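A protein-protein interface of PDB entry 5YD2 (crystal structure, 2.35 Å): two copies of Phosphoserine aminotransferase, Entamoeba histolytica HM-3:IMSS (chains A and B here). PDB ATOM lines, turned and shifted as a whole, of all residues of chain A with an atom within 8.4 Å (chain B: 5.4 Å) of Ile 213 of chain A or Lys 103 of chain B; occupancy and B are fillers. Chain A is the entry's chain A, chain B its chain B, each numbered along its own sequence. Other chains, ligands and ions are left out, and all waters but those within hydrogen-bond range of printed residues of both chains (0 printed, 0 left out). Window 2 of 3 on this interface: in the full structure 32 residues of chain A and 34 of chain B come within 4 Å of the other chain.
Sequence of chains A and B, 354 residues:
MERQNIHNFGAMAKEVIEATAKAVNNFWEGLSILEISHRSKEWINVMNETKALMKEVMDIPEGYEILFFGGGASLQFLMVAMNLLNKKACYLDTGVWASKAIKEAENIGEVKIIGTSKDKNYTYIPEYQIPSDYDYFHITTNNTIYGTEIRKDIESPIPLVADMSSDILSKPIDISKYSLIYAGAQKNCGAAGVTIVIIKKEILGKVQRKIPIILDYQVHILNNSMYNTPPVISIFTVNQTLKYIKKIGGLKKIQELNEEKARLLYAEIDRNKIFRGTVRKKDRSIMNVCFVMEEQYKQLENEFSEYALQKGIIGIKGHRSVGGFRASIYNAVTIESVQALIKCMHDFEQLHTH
Of chain B, only Lys 103, Glu 104 and Asn 107 come within 4 Å of Ile 213 of chain A. Lys 103 of chain B touches one residue of chain A. Of the printed residues of chain B, Ile 214 of chain A touches Glu 104 (2.9 Å). Of the printed residues of chain B, Pro 212 of chain A touches Glu 104. Printed residues of chain A within 4 Å of Glu 104 of chain B: Pro 212 (3.3 Å), Ile 213 (2.8 Å) and Ile 214 (2.9 Å). Of the printed residues of chain A, Lys 100 of chain B touches Tyr 227. Printed residues of chain A within 4 Å of Asn 107 of chain B: Ile 213 (3.9 Å). Ser 99 of chain B touches none of the printed residues of chain A. The nearest printed residue of chain B that does not touch Ile 213 of chain A is Lys 100 of chain B (5.9 Å). The nearest printed residue of chain B that does not touch Ile 214 of chain A is Asn 107 of chain B (6.8 Å).
Among the printed residues, pairs that only touch across the chains: Pro 212 of chain A with Glu 104 of chain B (3.3 Å), Tyr 227 of chain A with Lys 100 of chain B (3.8 Å), Ile 213 of chain A with Lys 103 of chain B (3.8 Å) and Ile 213 of chain A with Asn 107 of chain B (3.9 Å).
The backbone carbonyl oxygen (O) of Ile 214 of chain A is in hydrogen-bond range of a ring nitrogen (NE2) of His 220 of chain A, at 2.8 Å. The side-chain amide nitrogen (ND2) of Asn 107 of chain B is in hydrogen-bond range of the side-chain carboxylate (OE1) of Glu 104 of chain B, at 3.3 Å.
No position is printed for both chains. Of the 6 pairs that touch across the chains among the printed residues, none has its exchanged pair printed and touching as well.
The backbone NH of Ile 214 of chain A lies within hydrogen-bond range of the side-chain carboxylate of Glu 104 of chain B (2.9 Å). The side-chain carboxylate (OE1) of Glu 104 of chain B is in hydrogen-bond range of the backbone NH (N) of Ile 213 of chain A, at 2.8 Å.
Of the 16 printed residues of chain A, 4 touch a printed residue of chain B. Among the printed residues, 6 pairs touch across the chains. Among the printed residues, no Asp or Glu carboxylate lies within 4 Å of a Lys or Arg side-chain nitrogen of the other chain.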
ATOM      1  N   PHE A  69      13.377  10.635  20.608  1.00  0.00           N
ATOM      2  CA  PHE A  69      13.933   9.766  19.629  1.00  0.00           C
ATOM      3  C   PHE A  69      15.348  10.164  19.433  1.00  0.00           C
ATOM      4  O   PHE A  69      15.710  11.335  19.450  1.00  0.00           O
ATOM      5  CB  PHE A  69      13.197   9.904  18.319  1.00  0.00           C
ATOM      6  CG  PHE A  69      11.835   9.269  18.314  1.00  0.00           C
ATOM      7  CD1 PHE A  69      11.683   7.961  17.934  1.00  0.00           C
ATOM      8  CD2 PHE A  69      10.732   9.994  18.586  1.00  0.00           C
ATOM      9  CE1 PHE A  69      10.460   7.384  17.861  1.00  0.00           C
ATOM     10  CE2 PHE A  69       9.491   9.432  18.529  1.00  0.00           C
ATOM     11  CZ  PHE A  69       9.339   8.129  18.156  1.00  0.00           C
ATOM     12  N   MET A  79       8.922   9.083   9.532  1.00  0.00           N
ATOM     13  CA  MET A  79       7.935   8.567  10.497  1.00  0.00           C
ATOM     14  C   MET A  79       6.609   9.248  10.353  1.00  0.00           C
ATOM     15  O   MET A  79       5.564   8.576  10.358  1.00  0.00           O
ATOM     16  CB  MET A  79       8.435   8.691  11.912  1.00  0.00           C
ATOM     17  CG  MET A  79       9.593   7.738  12.148  1.00  0.00           C
ATOM     18  SD  MET A  79      10.193   7.677  13.827  1.00  0.00           S
ATOM     19  CE  MET A  79       8.743   7.046  14.668  1.00  0.00           C
ATOM     20  N   ASN A  83       3.341   6.879   9.544  1.00  0.00           N
ATOM     21  CA  ASN A  83       2.301   6.796  10.526  1.00  0.00           C
ATOM     22  C   ASN A  83       0.991   7.511  10.208  1.00  0.00           C
ATOM     23  O   ASN A  83      -0.035   7.120  10.802  1.00  0.00           O
ATOM     24  CB  ASN A  83       2.822   7.285  11.856  1.00  0.00           C
ATOM     25  CG  ASN A  83       3.800   6.330  12.470  1.00  0.00           C
ATOM     26  OD1 ASN A  83       3.449   5.591  13.340  1.00  0.00           O
ATOM     27  ND2 ASN A  83       5.024   6.333  11.998  1.00  0.00           N
ATOM     28  N   LYS A 210       1.554  -1.292   6.322  1.00  0.00           N
ATOM     29  CA  LYS A 210       2.378  -1.848   7.388  1.00  0.00           C
ATOM     30  C   LYS A 210       3.447  -0.836   7.771  1.00  0.00           C
ATOM     31  O   LYS A 210       4.018  -0.175   6.920  1.00  0.00           O
ATOM     32  CB  LYS A 210       3.134  -3.113   6.921  1.00  0.00           C
ATOM     33  CG  LYS A 210       2.497  -3.925   5.781  1.00  0.00           C
ATOM     34  CD  LYS A 210       1.042  -4.289   6.134  1.00  0.00           C
ATOM     35  CE  LYS A 210       0.354  -5.106   5.050  1.00  0.00           C
ATOM     36  NZ  LYS A 210      -1.060  -5.394   5.406  1.00  0.00           N
ATOM     37  N   ILE A 211       3.730  -0.714   9.048  1.00  0.00           N
ATOM     38  CA  ILE A 211       4.785   0.142   9.499  1.00  0.00           C
ATOM     39  C   ILE A 211       5.804  -0.685  10.251  1.00  0.00           C
ATOM     40  O   ILE A 211       5.456  -1.373  11.188  1.00  0.00           O
ATOM     41  CB  ILE A 211       4.267   1.185  10.493  1.00  0.00           C
ATOM     42  CG1 ILE A 211       3.058   1.921   9.930  1.00  0.00           C
ATOM     43  CG2 ILE A 211       5.398   2.146  10.831  1.00  0.00           C
ATOM     44  CD1 ILE A 211       2.363   2.769  10.953  1.00  0.00           C
ATOM     45  N   PRO A 212       7.071  -0.572   9.890  1.00  0.00           N
ATOM     46  CA  PRO A 212       8.088  -1.200  10.674  1.00  0.00           C
ATOM     47  C   PRO A 212       7.967  -0.799  12.131  1.00  0.00           C
ATOM     48  O   PRO A 212       7.685   0.357  12.455  1.00  0.00           O
ATOM     49  CB  PRO A 212       9.375  -0.619  10.083  1.00  0.00           C
ATOM     50  CG  PRO A 212       9.052  -0.428   8.628  1.00  0.00           C
ATOM     51  CD  PRO A 212       7.600  -0.029   8.623  1.00  0.00           C
ATOM     52  N   ILE A 213       8.235  -1.765  12.994  1.00  0.00           N
ATOM     53  CA  ILE A 213       8.121  -1.615  14.424  1.00  0.00           C
ATOM     54  C   ILE A 213       8.914  -0.438  14.961  1.00  0.00           C
ATOM     55  O   ILE A 213       8.409   0.372  15.736  1.00  0.00           O
ATOM     56  CB  ILE A 213       8.568  -2.940  15.094  1.00  0.00           C
ATOM     57  CG1 ILE A 213       7.466  -4.011  14.884  1.00  0.00           C
ATOM     58  CG2 ILE A 213       8.890  -2.751  16.562  1.00  0.00           C
ATOM     59  CD1 ILE A 213       7.954  -5.459  14.982  1.00  0.00           C
ATOM     60  N   ILE A 214      10.155  -0.328  14.533  1.00  0.00           N
ATOM     61  CA  ILE A 214      10.987   0.780  15.000  1.00  0.00           C
ATOM     62  C   ILE A 214      10.504   2.158  14.484  1.00  0.00           C
ATOM     63  O   ILE A 214      10.810   3.166  15.097  1.00  0.00           O
ATOM     64  CB  ILE A 214      12.452   0.530  14.667  1.00  0.00           C
ATOM     65  CG1 ILE A 214      13.395   1.473  15.443  1.00  0.00           C
ATOM     66  CG2 ILE A 214      12.694   0.649  13.167  1.00  0.00           C
ATOM     67  CD1 ILE A 214      13.230   1.463  16.940  1.00  0.00           C
ATOM     68  N   LEU A 215       9.674   2.194  13.450  1.00  0.00           N
ATOM     69  CA  LEU A 215       9.124   3.440  12.977  1.00  0.00           C
ATOM     70  C   LEU A 215       7.690   3.735  13.405  1.00  0.00           C
ATOM     71  O   LEU A 215       7.082   4.670  12.905  1.00  0.00           O
ATOM     72  CB  LEU A 215       9.171   3.431  11.449  1.00  0.00           C
ATOM     73  CG  LEU A 215      10.574   3.355  10.838  1.00  0.00           C
ATOM     74  CD1 LEU A 215      10.523   3.482   9.325  1.00  0.00           C
ATOM     75  CD2 LEU A 215      11.493   4.397  11.412  1.00  0.00           C
ATOM     76  N   ASP A 216       7.122   2.933  14.289  1.00  0.00           N
ATOM     77  CA  ASP A 216       5.692   2.978  14.596  1.00  0.00           C
ATOM     78  C   ASP A 216       5.561   3.787  15.874  1.00  0.00           C
ATOM     79  O   ASP A 216       6.049   3.339  16.921  1.00  0.00           O
ATOM     80  CB  ASP A 216       5.175   1.533  14.797  1.00  0.00           C
ATOM     81  CG  ASP A 216       3.647   1.449  15.008  1.00  0.00           C
ATOM     82  OD1 ASP A 216       3.028   2.358  15.552  1.00  0.00           O
ATOM     83  OD2 ASP A 216       3.024   0.449  14.630  1.00  0.00           O
ATOM     84  N   TYR A 217       4.914   4.949  15.818  1.00  0.00           N
ATOM     85  CA  TYR A 217       4.821   5.798  17.020  1.00  0.00           C
ATOM     86  C   TYR A 217       4.104   5.071  18.200  1.00  0.00           C
ATOM     87  O   TYR A 217       4.450   5.264  19.370  1.00  0.00           O
ATOM     88  CB  TYR A 217       4.066   7.093  16.755  1.00  0.00           C
ATOM     89  CG  TYR A 217       4.778   8.152  15.905  1.00  0.00           C
ATOM     90  CD1 TYR A 217       5.933   8.751  16.338  1.00  0.00           C
ATOM     91  CD2 TYR A 217       4.218   8.601  14.726  1.00  0.00           C
ATOM     92  CE1 TYR A 217       6.553   9.725  15.583  1.00  0.00           C
ATOM     93  CE2 TYR A 217       4.859   9.547  13.953  1.00  0.00           C
ATOM     94  CZ  TYR A 217       6.023  10.104  14.391  1.00  0.00           C
ATOM     95  OH  TYR A 217       6.636  11.063  13.651  1.00  0.00           O
ATOM     96  N   GLN A 218       3.117   4.242  17.889  1.00  0.00           N
ATOM     97  CA  GLN A 218       2.425   3.458  18.919  1.00  0.00           C
ATOM     98  C   GLN A 218       3.361   2.563  19.734  1.00  0.00           C
ATOM     99  O   GLN A 218       3.298   2.551  20.965  1.00  0.00           O
ATOM    100  CB  GLN A 218       1.335   2.613  18.314  1.00  0.00           C
ATOM    101  CG  GLN A 218       0.225   3.442  17.704  1.00  0.00           C
ATOM    102  CD  GLN A 218      -0.893   2.513  17.231  1.00  0.00           C
ATOM    103  OE1 GLN A 218      -1.613   1.904  18.042  1.00  0.00           O
ATOM    104  NE2 GLN A 218      -1.015   2.360  15.908  1.00  0.00           N
ATOM    105  N   VAL A 219       4.250   1.845  19.069  1.00  0.00           N
ATOM    106  CA  VAL A 219       5.160   1.047  19.804  1.00  0.00           C
ATOM    107  C   VAL A 219       5.973   1.872  20.754  1.00  0.00           C
ATOM    108  O   VAL A 219       6.220   1.466  21.892  1.00  0.00           O
ATOM    109  CB  VAL A 219       6.048   0.258  18.885  1.00  0.00           C
ATOM    110  CG1 VAL A 219       7.206  -0.384  19.683  1.00  0.00           C
ATOM    111  CG2 VAL A 219       5.197  -0.775  18.144  1.00  0.00           C
ATOM    112  N   HIS A 220       6.368   3.066  20.325  1.00  0.00           N
ATOM    113  CA  HIS A 220       7.127   3.966  21.211  1.00  0.00           C
ATOM    114  C   HIS A 220       6.322   4.474  22.399  1.00  0.00           C
ATOM    115  O   HIS A 220       6.848   4.622  23.503  1.00  0.00           O
ATOM    116  CB  HIS A 220       7.755   5.125  20.400  1.00  0.00           C
ATOM    117  CG  HIS A 220       8.762   4.648  19.418  1.00  0.00           C
ATOM    118  ND1 HIS A 220      10.015   4.230  19.802  1.00  0.00           N
ATOM    119  CD2 HIS A 220       8.663   4.381  18.093  1.00  0.00           C
ATOM    120  CE1 HIS A 220      10.677   3.814  18.739  1.00  0.00           C
ATOM    121  NE2 HIS A 220       9.881   3.895  17.685  1.00  0.00           N
ATOM    122  N   ASN A 223       5.830   2.044  25.144  1.00  0.00           N
ATOM    123  CA  ASN A 223       7.001   1.858  25.963  1.00  0.00           C
ATOM    124  C   ASN A 223       7.584   3.089  26.521  1.00  0.00           C
ATOM    125  O   ASN A 223       8.704   3.047  26.958  1.00  0.00           O
ATOM    126  CB  ASN A 223       8.045   1.135  25.172  1.00  0.00           C
ATOM    127  CG  ASN A 223       7.615  -0.266  24.811  1.00  0.00           C
ATOM    128  OD1 ASN A 223       8.037  -1.214  25.445  1.00  0.00           O
ATOM    129  ND2 ASN A 223       6.793  -0.406  23.792  1.00  0.00           N
ATOM    130  N   TYR A 227      11.179   1.813  24.189  1.00  0.00           N
ATOM    131  CA  TYR A 227      11.109   0.628  23.372  1.00  0.00           C
ATOM    132  C   TYR A 227      12.513   0.104  23.177  1.00  0.00           C
ATOM    133  O   TYR A 227      12.765  -1.083  23.283  1.00  0.00           O
ATOM    134  CB  TYR A 227      10.510   0.878  21.997  1.00  0.00           C
ATOM    135  CG  TYR A 227      10.616  -0.365  21.176  1.00  0.00           C
ATOM    136  CD1 TYR A 227       9.868  -1.476  21.513  1.00  0.00           C
ATOM    137  CD2 TYR A 227      11.502  -0.475  20.132  1.00  0.00           C
ATOM    138  CE1 TYR A 227       9.956  -2.649  20.805  1.00  0.00           C
ATOM    139  CE2 TYR A 227      11.599  -1.628  19.406  1.00  0.00           C
ATOM    140  CZ  TYR A 227      10.815  -2.723  19.754  1.00  0.00           C
ATOM    141  OH  TYR A 227      10.874  -3.930  19.099  1.00  0.00           O
ATOM    142  N   ALA B  98      18.154 -11.354  18.340  1.00  0.00           N
ATOM    143  CA  ALA B  98      18.094 -12.038  17.059  1.00  0.00           C
ATOM    144  C   ALA B  98      16.662 -12.135  16.571  1.00  0.00           C
ATOM    145  O   ALA B  98      16.394 -11.940  15.393  1.00  0.00           O
ATOM    146  CB  ALA B  98      18.674 -13.411  17.170  1.00  0.00           C
ATOM    147  N   SER B  99      15.742 -12.419  17.492  1.00  0.00           N
ATOM    148  CA  SER B  99      14.362 -12.591  17.135  1.00  0.00           C
ATOM    149  C   SER B  99      13.713 -11.289  16.712  1.00  0.00           C
ATOM    150  O   SER B  99      12.852 -11.255  15.836  1.00  0.00           O
ATOM    151  CB  SER B  99      13.642 -13.221  18.340  1.00  0.00           C
ATOM    152  OG  SER B  99      12.248 -13.135  18.217  1.00  0.00           O
ATOM    153  N   LYS B 100      14.084 -10.200  17.356  1.00  0.00           N
ATOM    154  CA  LYS B 100      13.559  -8.911  16.984  1.00  0.00           C
ATOM    155  C   LYS B 100      14.109  -8.468  15.609  1.00  0.00           C
ATOM    156  O   LYS B 100      13.389  -7.863  14.835  1.00  0.00           O
ATOM    157  CB  LYS B 100      13.919  -7.908  18.055  1.00  0.00           C
ATOM    158  CG  LYS B 100      12.996  -7.934  19.255  1.00  0.00           C
ATOM    159  CD  LYS B 100      13.465  -6.909  20.278  1.00  0.00           C
ATOM    160  CE  LYS B 100      12.404  -6.606  21.316  1.00  0.00           C
ATOM    161  NZ  LYS B 100      12.825  -5.423  22.123  1.00  0.00           N
ATOM    162  N   ALA B 101      15.359  -8.797  15.302  1.00  0.00           N
ATOM    163  CA  ALA B 101      15.905  -8.519  13.966  1.00  0.00           C
ATOM    164  C   ALA B 101      15.095  -9.245  12.909  1.00  0.00           C
ATOM    165  O   ALA B 101      14.740  -8.661  11.886  1.00  0.00           O
ATOM    166  CB  ALA B 101      17.362  -8.928  13.870  1.00  0.00           C
ATOM    167  N   ILE B 102      14.810 -10.528  13.181  1.00  0.00           N
ATOM    168  CA  ILE B 102      14.135 -11.398  12.243  1.00  0.00           C
ATOM    169  C   ILE B 102      12.775 -10.846  11.917  1.00  0.00           C
ATOM    170  O   ILE B 102      12.394 -10.773  10.783  1.00  0.00           O
ATOM    171  CB  ILE B 102      13.969 -12.788  12.864  1.00  0.00           C
ATOM    172  CG1 ILE B 102      15.233 -13.591  12.629  1.00  0.00           C
ATOM    173  CG2 ILE B 102      12.766 -13.551  12.298  1.00  0.00           C
ATOM    174  CD1 ILE B 102      15.255 -14.833  13.491  1.00  0.00           C
ATOM    175  N   LYS B 103      12.038 -10.487  12.940  1.00  0.00           N
ATOM    176  CA  LYS B 103      10.728  -9.899  12.801  1.00  0.00           C
ATOM    177  C   LYS B 103      10.731  -8.600  11.988  1.00  0.00           C
ATOM    178  O   LYS B 103       9.863  -8.395  11.132  1.00  0.00           O
ATOM    179  CB  LYS B 103      10.183  -9.611  14.208  1.00  0.00           C
ATOM    180  CG  LYS B 103       8.753  -9.135  14.262  1.00  0.00           C
ATOM    181  CD  LYS B 103       7.808 -10.322  14.371  1.00  0.00           C
ATOM    182  CE  LYS B 103       6.346  -9.853  14.479  1.00  0.00           C
ATOM    183  NZ  LYS B 103       5.467 -10.972  14.927  1.00  0.00           N
ATOM    184  N   GLU B 104      11.676  -7.710  12.239  1.00  0.00           N
ATOM    185  CA  GLU B 104      11.671  -6.446  11.505  1.00  0.00           C
ATOM    186  C   GLU B 104      11.905  -6.751  10.069  1.00  0.00           C
ATOM    187  O   GLU B 104      11.244  -6.193   9.204  1.00  0.00           O
ATOM    188  CB  GLU B 104      12.684  -5.440  12.046  1.00  0.00           C
ATOM    189  CG  GLU B 104      12.441  -4.011  11.578  1.00  0.00           C
ATOM    190  CD  GLU B 104      11.266  -3.303  12.226  1.00  0.00           C
ATOM    191  OE1 GLU B 104      10.095  -3.578  11.857  1.00  0.00           O
ATOM    192  OE2 GLU B 104      11.507  -2.446  13.097  1.00  0.00           O
ATOM    193  N   ALA B 105      12.839  -7.657   9.811  1.00  0.00           N
ATOM    194  CA  ALA B 105      13.168  -8.067   8.445  1.00  0.00           C
ATOM    195  C   ALA B 105      11.995  -8.737   7.744  1.00  0.00           C
ATOM    196  O   ALA B 105      11.831  -8.596   6.535  1.00  0.00           O
ATOM    197  CB  ALA B 105      14.360  -9.005   8.453  1.00  0.00           C
ATOM    198  N   GLU B 106      11.212  -9.502   8.496  1.00  0.00           N
ATOM    199  CA  GLU B 106      10.046 -10.190   7.927  1.00  0.00           C
ATOM    200  C   GLU B 106       9.003  -9.192   7.448  1.00  0.00           C
ATOM    201  O   GLU B 106       8.309  -9.471   6.513  1.00  0.00           O
ATOM    202  CB  GLU B 106       9.398 -11.136   8.952  1.00  0.00           C
ATOM    203  CG  GLU B 106      10.143 -12.453   9.150  1.00  0.00           C
ATOM    204  CD  GLU B 106       9.541 -13.325  10.268  1.00  0.00           C
ATOM    205  OE1 GLU B 106       8.849 -12.781  11.175  1.00  0.00           O
ATOM    206  OE2 GLU B 106       9.762 -14.563  10.245  1.00  0.00           O
ATOM    207  N   ASN B 107       8.861  -8.068   8.134  1.00  0.00           N
ATOM    208  CA  ASN B 107       7.977  -6.986   7.683  1.00  0.00           C
ATOM    209  C   ASN B 107       8.414  -6.365   6.356  1.00  0.00           C
ATOM    210  O   ASN B 107       7.642  -5.640   5.748  1.00  0.00           O
ATOM    211  CB  ASN B 107       7.898  -5.851   8.716  1.00  0.00           C
ATOM    212  CG  ASN B 107       7.195  -6.258  10.006  1.00  0.00           C
ATOM    213  OD1 ASN B 107       6.256  -7.085   9.995  1.00  0.00           O
ATOM    214  ND2 ASN B 107       7.625  -5.642  11.140  1.00  0.00           N
